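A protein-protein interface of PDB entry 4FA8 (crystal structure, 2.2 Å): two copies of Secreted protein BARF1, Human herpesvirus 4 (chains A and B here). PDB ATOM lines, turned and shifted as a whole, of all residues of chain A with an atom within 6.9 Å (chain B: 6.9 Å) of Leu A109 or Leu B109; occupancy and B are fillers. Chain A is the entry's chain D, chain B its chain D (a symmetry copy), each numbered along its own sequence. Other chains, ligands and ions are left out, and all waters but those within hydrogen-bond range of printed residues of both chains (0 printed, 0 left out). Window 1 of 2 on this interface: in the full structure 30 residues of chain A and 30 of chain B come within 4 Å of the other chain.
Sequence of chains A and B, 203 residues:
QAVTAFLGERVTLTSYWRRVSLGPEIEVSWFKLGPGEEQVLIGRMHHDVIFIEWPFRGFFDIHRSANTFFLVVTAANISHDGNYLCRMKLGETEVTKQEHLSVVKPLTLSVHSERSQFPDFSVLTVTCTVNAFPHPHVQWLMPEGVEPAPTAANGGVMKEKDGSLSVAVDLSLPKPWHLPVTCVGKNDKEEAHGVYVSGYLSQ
Leu A107 touches Val B111 (O to O, 3.6 Å).
Leu A107 touches His B112 (O to CB, 3.2 Å).
CB of His B112 touches OG1 of Thr A108, 3.5 Å away.
O of Leu A109 touches CA of Ser B110, 3.0 Å away.
CA of Ser A110 touches O of Leu B109, 3.0 Å away.
Leu B107 touches Val A111 (O to O, 3.6 Å).
Thr B108 touches Val A111 (CA to O, 3.3 Å).
His A193 touches Gly B194 (O to CA, 3.4 Å).
Gly A194 touches His B193 (CA to O, 3.4 Å).
Val A195 touches Ala B192 (O to CA, 2.9 Å).
Leu A109 touches just these residues of chain B: Leu B109, Ser B110 and Val B111.
Printed residues of chain B within 4 Å of Ala A192: Val B195 (2.9 Å).
Of the printed residues of chain B, Gly A194 touches His B193 (3.4 Å).
Printed residues of chain A within 4 Å of Leu B107: Val A111 and His A112.
Printed residues of chain A within 4 Å of Leu B109: Leu A109, Ser A110 and Val A111.
Of the printed residues of chain A, His B112 touches Leu A107 (3.2 Å) and Thr A108 (3.5 Å).
Of the printed residues of chain A, His B193 touches His A193 (3.9 Å), Gly A194 (3.4 Å) and Val A195 (2.6 Å).
The nearest residue of chain B that does not touch Leu A109 is His B112 (5.2 Å).
The nearest printed residue of chain A that does not touch His B112 is Leu A109 (5.2 Å).
Printed residues of chain B that touch a printed residue of chain A: Leu B107, Thr B108, Leu B109, Ser B110, Val B111, His B112, Ala B192, His B193, Gly B194 and Val B195.
Printed residues of chain A that touch a printed residue of chain B: Leu A107, Thr A108, Leu A109, Ser A110, Val A111, His A112, Ala A192, His A193, Gly A194 and Val A195.
Hydrophobic or aromatic side chains of chain A within 4 Å of the printed part of chain B: Val A111, His A112, Ala A192, His A193 and Val A195.
Along chain A the printed residues that touch a printed residue of chain B span positions 107 to 195.
Among the printed residues, 21 pairs touch across the chains.
Among the printed residues, no Asp or Glu carboxylate lies within 4 Å of a Lys or Arg side-chain nitrogen of the other chain.
SG of Cys B128 forms a disulfide with SG of Cys B183, at 2.0 Å.
The backbone NH (N) of Cys B183 is in hydrogen-bond range of the backbone carbonyl oxygen (O) of Gly B194.
The backbone NH (N) of Gly B185 is in hydrogen-bond range of the backbone carbonyl oxygen (O) of Ala B192 (2.8 Å).
The backbone carbonyl oxygen of Ser B110 sits at hydrogen-bond distance from the backbone NH of Thr B129, 2.9 Å away.
The backbone carbonyl oxygen (O) of Gly A194 is in hydrogen-bond range of the backbone NH (N) of Cys A183, at 2.8 Å.
O of Ala A192 sits at hydrogen-bond distance from N of Gly A185 (2.8 Å).
Leu A107 touches Val B111, and with the chains exchanged Val A111 touches Leu B107.
Leu A109 touches Ser B110, and with the chains exchanged Ser A110 touches Leu B109.
Ala A192 touches Val B195, and with the chains exchanged Val A195 touches Ala B192.
His A193 touches Gly B194, and with the chains exchanged Gly A194 touches His B193.
Positions printed for both chains: 107, 108, 109, 110, 111, 112, 128, 129, 130, 131, 137, 138, 183, 184, 185, 186, 192, 193, 194 and 195.
Of the 21 pairs that touch across the chains among the printed residues, 21 have their exchanged pair printed and touching as well.
The side-chain hydroxyl of Ser A110 is in hydrogen-bond range of the side-chain hydroxyl of Ser B110 (3.2 Å).
The backbone carbonyl oxygen of Val A195 is in hydrogen-bond range of the backbone NH of His B193, 2.6 Å away.
O of Leu A109 sits close to O of Leu B109, at 3.5 Å.
The backbone NH (N) of His A193 sits at hydrogen-bond distance from the backbone carbonyl oxygen (O) of Val B195, 2.6 Å away.
The backbone NH (N) of Val A111 is in hydrogen-bond range of the backbone carbonyl oxygen (O) of Leu B109 (2.9 Å).
The backbone carbonyl oxygen of Leu A109 sits at hydrogen-bond distance from the backbone NH of Val B111.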
ATOM      1  N   LEU A 107       0.714 -18.280  21.199  1.00  0.00           N
ATOM      2  CA  LEU A 107      -0.082 -19.381  20.671  1.00  0.00           C
ATOM      3  C   LEU A 107       0.048 -20.666  21.479  1.00  0.00           C
ATOM      4  O   LEU A 107       1.093 -20.924  22.068  1.00  0.00           O
ATOM      5  CB  LEU A 107       0.205 -19.635  19.189  1.00  0.00           C
ATOM      6  CG  LEU A 107       1.542 -20.180  18.693  1.00  0.00           C
ATOM      7  CD1 LEU A 107       1.612 -21.696  18.799  1.00  0.00           C
ATOM      8  CD2 LEU A 107       1.716 -19.752  17.249  1.00  0.00           C
ATOM      9  N   THR A 108      -1.043 -21.437  21.512  1.00  0.00           N
ATOM     10  CA  THR A 108      -1.026 -22.843  21.923  1.00  0.00           C
ATOM     11  C   THR A 108      -1.337 -23.717  20.712  1.00  0.00           C
ATOM     12  O   THR A 108      -2.364 -23.530  20.039  1.00  0.00           O
ATOM     13  CB  THR A 108      -2.034 -23.151  23.052  1.00  0.00           C
ATOM     14  OG1 THR A 108      -1.847 -22.228  24.128  1.00  0.00           O
ATOM     15  CG2 THR A 108      -1.836 -24.576  23.584  1.00  0.00           C
ATOM     16  N   LEU A 109      -0.435 -24.649  20.420  1.00  0.00           N
ATOM     17  CA  LEU A 109      -0.671 -25.648  19.379  1.00  0.00           C
ATOM     18  C   LEU A 109      -0.931 -27.013  20.000  1.00  0.00           C
ATOM     19  O   LEU A 109      -0.169 -27.459  20.866  1.00  0.00           O
ATOM     20  CB  LEU A 109       0.510 -25.720  18.402  1.00  0.00           C
ATOM     21  CG  LEU A 109       0.411 -26.777  17.287  1.00  0.00           C
ATOM     22  CD1 LEU A 109       0.862 -26.223  15.945  1.00  0.00           C
ATOM     23  CD2 LEU A 109       1.191 -28.034  17.649  1.00  0.00           C
ATOM     24  N   SER A 110      -2.001 -27.662  19.541  1.00  0.00           N
ATOM     25  CA  SER A 110      -2.369 -29.015  19.961  1.00  0.00           C
ATOM     26  C   SER A 110      -2.488 -29.955  18.780  1.00  0.00           C
ATOM     27  O   SER A 110      -2.973 -29.567  17.710  1.00  0.00           O
ATOM     28  CB  SER A 110      -3.708 -29.001  20.696  1.00  0.00           C
ATOM     29  OG  SER A 110      -3.681 -28.088  21.786  1.00  0.00           O
ATOM     30  N   VAL A 111      -2.040 -31.191  18.979  1.00  0.00           N
ATOM     31  CA  VAL A 111      -2.313 -32.300  18.058  1.00  0.00           C
ATOM     32  C   VAL A 111      -2.830 -33.537  18.783  1.00  0.00           C
ATOM     33  O   VAL A 111      -2.325 -33.915  19.853  1.00  0.00           O
ATOM     34  CB  VAL A 111      -1.089 -32.713  17.207  1.00  0.00           C
ATOM     35  CG1 VAL A 111      -0.873 -31.732  16.067  1.00  0.00           C
ATOM     36  CG2 VAL A 111       0.160 -32.835  18.061  1.00  0.00           C
ATOM     37  N   HIS A 112      -3.845 -34.156  18.190  1.00  0.00           N
ATOM     38  CA  HIS A 112      -4.342 -35.445  18.639  1.00  0.00           C
ATOM     39  C   HIS A 112      -4.936 -36.134  17.460  1.00  0.00           C
ATOM     40  O   HIS A 112      -5.304 -35.485  16.475  1.00  0.00           O
ATOM     41  CB  HIS A 112      -5.381 -35.274  19.732  1.00  0.00           C
ATOM     42  CG  HIS A 112      -6.596 -34.490  19.301  1.00  0.00           C
ATOM     43  ND1 HIS A 112      -7.811 -35.057  19.161  1.00  0.00           N
ATOM     44  CD2 HIS A 112      -6.751 -33.142  18.980  1.00  0.00           C
ATOM     45  CE1 HIS A 112      -8.699 -34.122  18.767  1.00  0.00           C
ATOM     46  NE2 HIS A 112      -8.049 -32.951  18.657  1.00  0.00           N
ATOM     47  N   CYS A 128      -5.191 -30.571  14.277  1.00  0.00           N
ATOM     48  CA  CYS A 128      -4.288 -29.566  14.790  1.00  0.00           C
ATOM     49  C   CYS A 128      -5.032 -28.277  15.118  1.00  0.00           C
ATOM     50  O   CYS A 128      -5.756 -27.730  14.279  1.00  0.00           O
ATOM     51  CB  CYS A 128      -3.187 -29.303  13.788  1.00  0.00           C
ATOM     52  SG  CYS A 128      -1.788 -28.439  14.506  1.00  0.00           S
ATOM     53  N   THR A 129      -4.846 -27.808  16.349  1.00  0.00           N
ATOM     54  CA  THR A 129      -5.571 -26.657  16.870  1.00  0.00           C
ATOM     55  C   THR A 129      -4.595 -25.561  17.252  1.00  0.00           C
ATOM     56  O   THR A 129      -3.577 -25.822  17.897  1.00  0.00           O
ATOM     57  CB  THR A 129      -6.407 -27.046  18.105  1.00  0.00           C
ATOM     58  OG1 THR A 129      -7.124 -28.255  17.834  1.00  0.00           O
ATOM     59  CG2 THR A 129      -7.398 -25.951  18.458  1.00  0.00           C
ATOM     60  N   VAL A 130      -4.894 -24.336  16.831  1.00  0.00           N
ATOM     61  CA  VAL A 130      -4.118 -23.178  17.276  1.00  0.00           C
ATOM     62  C   VAL A 130      -5.018 -22.108  17.889  1.00  0.00           C
ATOM     63  O   VAL A 130      -5.966 -21.622  17.248  1.00  0.00           O
ATOM     64  CB  VAL A 130      -3.214 -22.601  16.157  1.00  0.00           C
ATOM     65  CG1 VAL A 130      -2.567 -21.294  16.594  1.00  0.00           C
ATOM     66  CG2 VAL A 130      -2.137 -23.606  15.773  1.00  0.00           C
ATOM     67  N   ASN A 131      -4.724 -21.789  19.150  1.00  0.00           N
ATOM     68  CA  ASN A 131      -5.310 -20.659  19.867  1.00  0.00           C
ATOM     69  C   ASN A 131      -4.266 -19.570  20.065  1.00  0.00           C
ATOM     70  O   ASN A 131      -3.174 -19.840  20.573  1.00  0.00           O
ATOM     71  CB  ASN A 131      -5.840 -21.087  21.234  1.00  0.00           C
ATOM     72  CG  ASN A 131      -6.449 -19.930  22.011  1.00  0.00           C
ATOM     73  OD1 ASN A 131      -5.886 -19.467  23.007  1.00  0.00           O
ATOM     74  ND2 ASN A 131      -7.599 -19.448  21.551  1.00  0.00           N
ATOM     75  N   HIS A 137      -3.374 -19.111  13.011  1.00  0.00           N
ATOM     76  CA  HIS A 137      -3.448 -19.690  11.673  1.00  0.00           C
ATOM     77  C   HIS A 137      -2.834 -21.057  11.707  1.00  0.00           C
ATOM     78  O   HIS A 137      -1.706 -21.221  12.177  1.00  0.00           O
ATOM     79  CB  HIS A 137      -2.740 -18.778  10.670  1.00  0.00           C
ATOM     80  CG  HIS A 137      -2.568 -19.376   9.292  1.00  0.00           C
ATOM     81  ND1 HIS A 137      -3.353 -19.033   8.250  1.00  0.00           N
ATOM     82  CD2 HIS A 137      -1.640 -20.297   8.797  1.00  0.00           C
ATOM     83  CE1 HIS A 137      -2.964 -19.707   7.149  1.00  0.00           C
ATOM     84  NE2 HIS A 137      -1.915 -20.478   7.483  1.00  0.00           N
ATOM     85  N   VAL A 138      -3.579 -22.053  11.226  1.00  0.00           N
ATOM     86  CA  VAL A 138      -3.100 -23.432  11.187  1.00  0.00           C
ATOM     87  C   VAL A 138      -3.109 -23.963   9.765  1.00  0.00           C
ATOM     88  O   VAL A 138      -3.915 -23.534   8.929  1.00  0.00           O
ATOM     89  CB  VAL A 138      -3.987 -24.413  11.992  1.00  0.00           C
ATOM     90  CG1 VAL A 138      -3.124 -25.327  12.842  1.00  0.00           C
ATOM     91  CG2 VAL A 138      -5.004 -23.696  12.852  1.00  0.00           C
ATOM     92  N   CYS A 183       1.994 -30.371  11.172  1.00  0.00           N
ATOM     93  CA  CYS A 183       1.100 -29.248  11.225  1.00  0.00           C
ATOM     94  C   CYS A 183       1.930 -27.996  11.509  1.00  0.00           C
ATOM     95  O   CYS A 183       2.888 -28.044  12.283  1.00  0.00           O
ATOM     96  CB  CYS A 183       0.087 -29.477  12.346  1.00  0.00           C
ATOM     97  SG  CYS A 183      -0.693 -27.949  12.878  1.00  0.00           S
ATOM     98  N   VAL A 184       1.567 -26.879  10.881  1.00  0.00           N
ATOM     99  CA  VAL A 184       2.232 -25.594  11.140  1.00  0.00           C
ATOM    100  C   VAL A 184       1.260 -24.569  11.722  1.00  0.00           C
ATOM    101  O   VAL A 184       0.242 -24.241  11.108  1.00  0.00           O
ATOM    102  CB  VAL A 184       2.932 -25.019   9.884  1.00  0.00           C
ATOM    103  CG1 VAL A 184       3.651 -23.715  10.211  1.00  0.00           C
ATOM    104  CG2 VAL A 184       3.922 -26.024   9.316  1.00  0.00           C
ATOM    105  N   GLY A 185       1.591 -24.080  12.913  1.00  0.00           N
ATOM    106  CA  GLY A 185       0.804 -23.069  13.597  1.00  0.00           C
ATOM    107  C   GLY A 185       1.566 -21.764  13.703  1.00  0.00           C
ATOM    108  O   GLY A 185       2.761 -21.751  14.006  1.00  0.00           O
ATOM    109  N   LYS A 186       0.867 -20.664  13.441  1.00  0.00           N
ATOM    110  CA  LYS A 186       1.462 -19.328  13.470  1.00  0.00           C
ATOM    111  C   LYS A 186       0.562 -18.346  14.200  1.00  0.00           C
ATOM    112  O   LYS A 186      -0.653 -18.536  14.252  1.00  0.00           O
ATOM    113  CB  LYS A 186       1.716 -18.831  12.049  1.00  0.00           C
ATOM    114  CG  LYS A 186       2.978 -19.374  11.413  1.00  0.00           C
ATOM    115  CD  LYS A 186       2.892 -19.267   9.901  1.00  0.00           C
ATOM    116  CE  LYS A 186       4.245 -18.953   9.286  1.00  0.00           C
ATOM    117  NZ  LYS A 186       4.662 -17.556   9.611  1.00  0.00           N
ATOM    118  N   ALA A 192       5.040 -22.482  15.618  1.00  0.00           N
ATOM    119  CA  ALA A 192       5.228 -23.773  16.251  1.00  0.00           C
ATOM    120  C   ALA A 192       4.772 -24.873  15.304  1.00  0.00           C
ATOM    121  O   ALA A 192       3.919 -24.657  14.440  1.00  0.00           O
ATOM    122  CB  ALA A 192       4.456 -23.840  17.562  1.00  0.00           C
ATOM    123  N   HIS A 193       5.355 -26.053  15.464  1.00  0.00           N
ATOM    124  CA  HIS A 193       4.937 -27.221  14.698  1.00  0.00           C
ATOM    125  C   HIS A 193       4.439 -28.325  15.588  1.00  0.00           C
ATOM    126  O   HIS A 193       4.922 -28.512  16.716  1.00  0.00           O
ATOM    127  CB  HIS A 193       6.079 -27.756  13.836  1.00  0.00           C
ATOM    128  CG  HIS A 193       6.651 -26.753  12.857  1.00  0.00           C
ATOM    129  ND1 HIS A 193       7.843 -26.936  12.256  1.00  0.00           N
ATOM    130  CD2 HIS A 193       6.154 -25.541  12.381  1.00  0.00           C
ATOM    131  CE1 HIS A 193       8.096 -25.901  11.439  1.00  0.00           C
ATOM    132  NE2 HIS A 193       7.064 -25.045  11.520  1.00  0.00           N
ATOM    133  N   GLY A 194       3.457 -29.063  15.079  1.00  0.00           N
ATOM    134  CA  GLY A 194       3.022 -30.309  15.688  1.00  0.00           C
ATOM    135  C   GLY A 194       3.315 -31.445  14.738  1.00  0.00           C
ATOM    136  O   GLY A 194       2.983 -31.364  13.551  1.00  0.00           O
ATOM    137  N   VAL A 195       3.959 -32.492  15.251  1.00  0.00           N
ATOM    138  CA  VAL A 195       4.293 -33.664  14.442  1.00  0.00           C
ATOM    139  C   VAL A 195       3.674 -34.923  15.037  1.00  0.00           C
ATOM    140  O   VAL A 195       3.920 -35.258  16.187  1.00  0.00           O
ATOM    141  CB  VAL A 195       5.818 -33.845  14.277  1.00  0.00           C
ATOM    142  CG1 VAL A 195       6.128 -35.035  13.381  1.00  0.00           C
ATOM    143  CG2 VAL A 195       6.444 -32.584  13.696  1.00  0.00           C
ATOM    144  N   LEU B 107      -3.276 -39.604  22.524  1.00  0.00           N
ATOM    145  CA  LEU B 107      -2.657 -38.461  23.184  1.00  0.00           C
ATOM    146  C   LEU B 107      -3.004 -37.126  22.539  1.00  0.00           C
ATOM    147  O   LEU B 107      -3.228 -37.060  21.335  1.00  0.00           O
ATOM    148  CB  LEU B 107      -1.141 -38.629  23.314  1.00  0.00           C
ATOM    149  CG  LEU B 107      -0.206 -38.615  22.107  1.00  0.00           C
ATOM    150  CD1 LEU B 107       0.151 -37.198  21.682  1.00  0.00           C
ATOM    151  CD2 LEU B 107       1.050 -39.377  22.479  1.00  0.00           C
ATOM    152  N   THR B 108      -3.070 -36.084  23.373  1.00  0.00           N
ATOM    153  CA  THR B 108      -3.041 -34.689  22.928  1.00  0.00           C
ATOM    154  C   THR B 108      -1.739 -34.046  23.396  1.00  0.00           C
ATOM    155  O   THR B 108      -1.413 -34.070  24.593  1.00  0.00           O
ATOM    156  CB  THR B 108      -4.238 -33.866  23.452  1.00  0.00           C
ATOM    157  OG1 THR B 108      -5.459 -34.548  23.151  1.00  0.00           O
ATOM    158  CG2 THR B 108      -4.273 -32.479  22.797  1.00  0.00           C
ATOM    159  N   LEU B 109      -0.985 -33.502  22.446  1.00  0.00           N
ATOM    160  CA  LEU B 109       0.214 -32.728  22.766  1.00  0.00           C
ATOM    161  C   LEU B 109      -0.029 -31.245  22.522  1.00  0.00           C
ATOM    162  O   LEU B 109      -0.523 -30.862  21.454  1.00  0.00           O
ATOM    163  CB  LEU B 109       1.421 -33.214  21.953  1.00  0.00           C
ATOM    164  CG  LEU B 109       2.737 -32.442  22.155  1.00  0.00           C
ATOM    165  CD1 LEU B 109       3.928 -33.379  22.266  1.00  0.00           C
ATOM    166  CD2 LEU B 109       2.950 -31.416  21.049  1.00  0.00           C
ATOM    167  N   SER B 110       0.331 -30.430  23.513  1.00  0.00           N
ATOM    168  CA  SER B 110       0.244 -28.971  23.433  1.00  0.00           C
ATOM    169  C   SER B 110       1.584 -28.316  23.700  1.00  0.00           C
ATOM    170  O   SER B 110       2.349 -28.770  24.559  1.00  0.00           O
ATOM    171  CB  SER B 110      -0.759 -28.438  24.454  1.00  0.00           C
ATOM    172  OG  SER B 110      -2.027 -29.061  24.295  1.00  0.00           O
ATOM    173  N   VAL B 111       1.863 -27.250  22.956  1.00  0.00           N
ATOM    174  CA  VAL B 111       2.973 -26.337  23.250  1.00  0.00           C
ATOM    175  C   VAL B 111       2.535 -24.877  23.240  1.00  0.00           C
ATOM    176  O   VAL B 111       1.772 -24.438  22.363  1.00  0.00           O
ATOM    177  CB  VAL B 111       4.171 -26.490  22.284  1.00  0.00           C
ATOM    178  CG1 VAL B 111       4.997 -27.714  22.644  1.00  0.00           C
ATOM    179  CG2 VAL B 111       3.710 -26.552  20.839  1.00  0.00           C
ATOM    180  N   HIS B 112       3.024 -24.135  24.227  1.00  0.00           N
ATOM    181  CA  HIS B 112       2.862 -22.692  24.272  1.00  0.00           C
ATOM    182  C   HIS B 112       4.014 -22.133  25.033  1.00  0.00           C
ATOM    183  O   HIS B 112       4.653 -22.846  25.815  1.00  0.00           O
ATOM    184  CB  HIS B 112       1.553 -22.314  24.940  1.00  0.00           C
ATOM    185  CG  HIS B 112       1.437 -22.787  26.368  1.00  0.00           C
ATOM    186  ND1 HIS B 112       1.444 -21.938  27.415  1.00  0.00           N
ATOM    187  CD2 HIS B 112       1.309 -24.069  26.902  1.00  0.00           C
ATOM    188  CE1 HIS B 112       1.328 -22.638  28.561  1.00  0.00           C
ATOM    189  NE2 HIS B 112       1.246 -23.941  28.245  1.00  0.00           N
ATOM    190  N   CYS B 128       5.297 -27.936  27.445  1.00  0.00           N
ATOM    191  CA  CYS B 128       4.745 -29.023  26.669  1.00  0.00           C
ATOM    192  C   CYS B 128       3.892 -29.939  27.538  1.00  0.00           C
ATOM    193  O   CYS B 128       4.341 -30.422  28.584  1.00  0.00           O
ATOM    194  CB  CYS B 128       5.860 -29.804  26.010  1.00  0.00           C
ATOM    195  SG  CYS B 128       5.276 -30.859  24.681  1.00  0.00           S
ATOM    196  N   THR B 129       2.659 -30.163  27.093  1.00  0.00           N
ATOM    197  CA  THR B 129       1.671 -30.914  27.856  1.00  0.00           C
ATOM    198  C   THR B 129       1.231 -32.135  27.072  1.00  0.00           C
ATOM    199  O   THR B 129       0.949 -32.046  25.875  1.00  0.00           O
ATOM    200  CB  THR B 129       0.439 -30.042  28.170  1.00  0.00           C
ATOM    201  OG1 THR B 129       0.870 -28.766  28.656  1.00  0.00           O
ATOM    202  CG2 THR B 129      -0.439 -30.700  29.220  1.00  0.00           C
ATOM    203  N   VAL B 130       1.196 -33.282  27.743  1.00  0.00           N
ATOM    204  CA  VAL B 130       0.633 -34.490  27.138  1.00  0.00           C
ATOM    205  C   VAL B 130      -0.458 -35.095  28.019  1.00  0.00           C
ATOM    206  O   VAL B 130      -0.229 -35.413  29.199  1.00  0.00           O
ATOM    207  CB  VAL B 130       1.719 -35.532  26.766  1.00  0.00           C
ATOM    208  CG1 VAL B 130       1.088 -36.844  26.316  1.00  0.00           C
ATOM    209  CG2 VAL B 130       2.620 -34.989  25.666  1.00  0.00           C
ATOM    210  N   ASN B 131      -1.651 -35.204  27.431  1.00  0.00           N
ATOM    211  CA  ASN B 131      -2.781 -35.933  28.000  1.00  0.00           C
ATOM    212  C   ASN B 131      -3.032 -37.207  27.208  1.00  0.00           C
ATOM    213  O   ASN B 131      -3.166 -37.161  25.982  1.00  0.00           O
ATOM    214  CB  ASN B 131      -4.051 -35.084  27.984  1.00  0.00           C
ATOM    215  CG  ASN B 131      -5.250 -35.818  28.562  1.00  0.00           C
ATOM    216  OD1 ASN B 131      -6.175 -36.197  27.837  1.00  0.00           O
ATOM    217  ND2 ASN B 131      -5.236 -36.035  29.873  1.00  0.00           N
ATOM    218  N   HIS B 137       3.590 -39.422  28.629  1.00  0.00           N
ATOM    219  CA  HIS B 137       4.980 -39.150  28.980  1.00  0.00           C
ATOM    220  C   HIS B 137       5.489 -38.046  28.104  1.00  0.00           C
ATOM    221  O   HIS B 137       5.368 -38.117  26.879  1.00  0.00           O
ATOM    222  CB  HIS B 137       5.815 -40.423  28.826  1.00  0.00           C
ATOM    223  CG  HIS B 137       7.306 -40.214  28.957  1.00  0.00           C
ATOM    224  ND1 HIS B 137       7.988 -40.533  30.077  1.00  0.00           N
ATOM    225  CD2 HIS B 137       8.252 -39.731  28.048  1.00  0.00           C
ATOM    226  CE1 HIS B 137       9.296 -40.255  29.906  1.00  0.00           C
ATOM    227  NE2 HIS B 137       9.458 -39.767  28.664  1.00  0.00           N
ATOM    228  N   VAL B 138       6.047 -37.007  28.725  1.00  0.00           N
ATOM    229  CA  VAL B 138       6.595 -35.868  27.994  1.00  0.00           C
ATOM    230  C   VAL B 138       8.066 -35.678  28.321  1.00  0.00           C
ATOM    231  O   VAL B 138       8.525 -36.026  29.416  1.00  0.00           O
ATOM    232  CB  VAL B 138       5.922 -34.522  28.359  1.00  0.00           C
ATOM    233  CG1 VAL B 138       5.602 -33.734  27.102  1.00  0.00           C
ATOM    234  CG2 VAL B 138       4.676 -34.709  29.196  1.00  0.00           C
ATOM    235  N   CYS B 183       9.822 -30.873  21.770  1.00  0.00           N
ATOM    236  CA  CYS B 183       9.236 -31.650  22.827  1.00  0.00           C
ATOM    237  C   CYS B 183       8.808 -32.997  22.241  1.00  0.00           C
ATOM    238  O   CYS B 183       8.331 -33.061  21.107  1.00  0.00           O
ATOM    239  CB  CYS B 183       8.023 -30.901  23.374  1.00  0.00           C
ATOM    240  SG  CYS B 183       6.903 -31.985  24.268  1.00  0.00           S
ATOM    241  N   VAL B 184       8.982 -34.069  23.012  1.00  0.00           N
ATOM    242  CA  VAL B 184       8.527 -35.403  22.595  1.00  0.00           C
ATOM    243  C   VAL B 184       7.461 -35.951  23.541  1.00  0.00           C
ATOM    244  O   VAL B 184       7.694 -36.096  24.744  1.00  0.00           O
ATOM    245  CB  VAL B 184       9.692 -36.414  22.452  1.00  0.00           C
ATOM    246  CG1 VAL B 184       9.183 -37.767  21.969  1.00  0.00           C
ATOM    247  CG2 VAL B 184      10.744 -35.886  21.489  1.00  0.00           C
ATOM    248  N   GLY B 185       6.294 -36.245  22.977  1.00  0.00           N
ATOM    249  CA  GLY B 185       5.180 -36.812  23.718  1.00  0.00           C
ATOM    250  C   GLY B 185       4.885 -38.226  23.262  1.00  0.00           C
ATOM    251  O   GLY B 185       4.884 -38.518  22.064  1.00  0.00           O
ATOM    252  N   LYS B 186       4.645 -39.107  24.228  1.00  0.00           N
ATOM    253  CA  LYS B 186       4.373 -40.518  23.958  1.00  0.00           C
ATOM    254  C   LYS B 186       3.198 -41.016  24.783  1.00  0.00           C
ATOM    255  O   LYS B 186       2.917 -40.476  25.852  1.00  0.00           O
ATOM    256  CB  LYS B 186       5.607 -41.362  24.262  1.00  0.00           C
ATOM    257  CG  LYS B 186       6.653 -41.360  23.168  1.00  0.00           C
ATOM    258  CD  LYS B 186       8.004 -41.762  23.731  1.00  0.00           C
ATOM    259  CE  LYS B 186       8.804 -42.579  22.731  1.00  0.00           C
ATOM    260  NZ  LYS B 186       8.198 -43.932  22.549  1.00  0.00           N
ATOM    261  N   ALA B 192       4.140 -38.146  19.301  1.00  0.00           N
ATOM    262  CA  ALA B 192       3.971 -36.860  18.654  1.00  0.00           C
ATOM    263  C   ALA B 192       5.059 -35.907  19.126  1.00  0.00           C
ATOM    264  O   ALA B 192       5.596 -36.050  20.227  1.00  0.00           O
ATOM    265  CB  ALA B 192       2.592 -36.290  18.956  1.00  0.00           C
ATOM    266  N   HIS B 193       5.390 -34.940  18.281  1.00  0.00           N
ATOM    267  CA  HIS B 193       6.339 -33.897  18.649  1.00  0.00           C
ATOM    268  C   HIS B 193       5.714 -32.531  18.600  1.00  0.00           C
ATOM    269  O   HIS B 193       4.837 -32.251  17.768  1.00  0.00           O
ATOM    270  CB  HIS B 193       7.564 -33.915  17.737  1.00  0.00           C
ATOM    271  CG  HIS B 193       8.318 -35.227  17.722  1.00  0.00           C
ATOM    272  ND1 HIS B 193       9.211 -35.532  16.759  1.00  0.00           N
ATOM    273  CD2 HIS B 193       8.291 -36.317  18.591  1.00  0.00           C
ATOM    274  CE1 HIS B 193       9.729 -36.748  16.998  1.00  0.00           C
ATOM    275  NE2 HIS B 193       9.161 -37.229  18.116  1.00  0.00           N
ATOM    276  N   GLY B 194       6.168 -31.669  19.506  1.00  0.00           N
ATOM    277  CA  GLY B 194       5.860 -30.250  19.454  1.00  0.00           C
ATOM    278  C   GLY B 194       7.139 -29.481  19.226  1.00  0.00           C
ATOM    279  O   GLY B 194       8.138 -29.718  19.913  1.00  0.00           O
ATOM    280  N   VAL B 195       7.118 -28.579  18.245  1.00  0.00           N
ATOM    281  CA  VAL B 195       8.286 -27.758  17.928  1.00  0.00           C
ATOM    282  C   VAL B 195       7.952 -26.277  18.048  1.00  0.00           C
ATOM    283  O   VAL B 195       7.041 -25.786  17.397  1.00  0.00           O
ATOM    284  CB  VAL B 195       8.853 -28.067  16.525  1.00  0.00           C
ATOM    285  CG1 VAL B 195      10.102 -27.240  16.252  1.00  0.00           C
ATOM    286  CG2 VAL B 195       9.177 -29.549  16.394  1.00  0.00           C
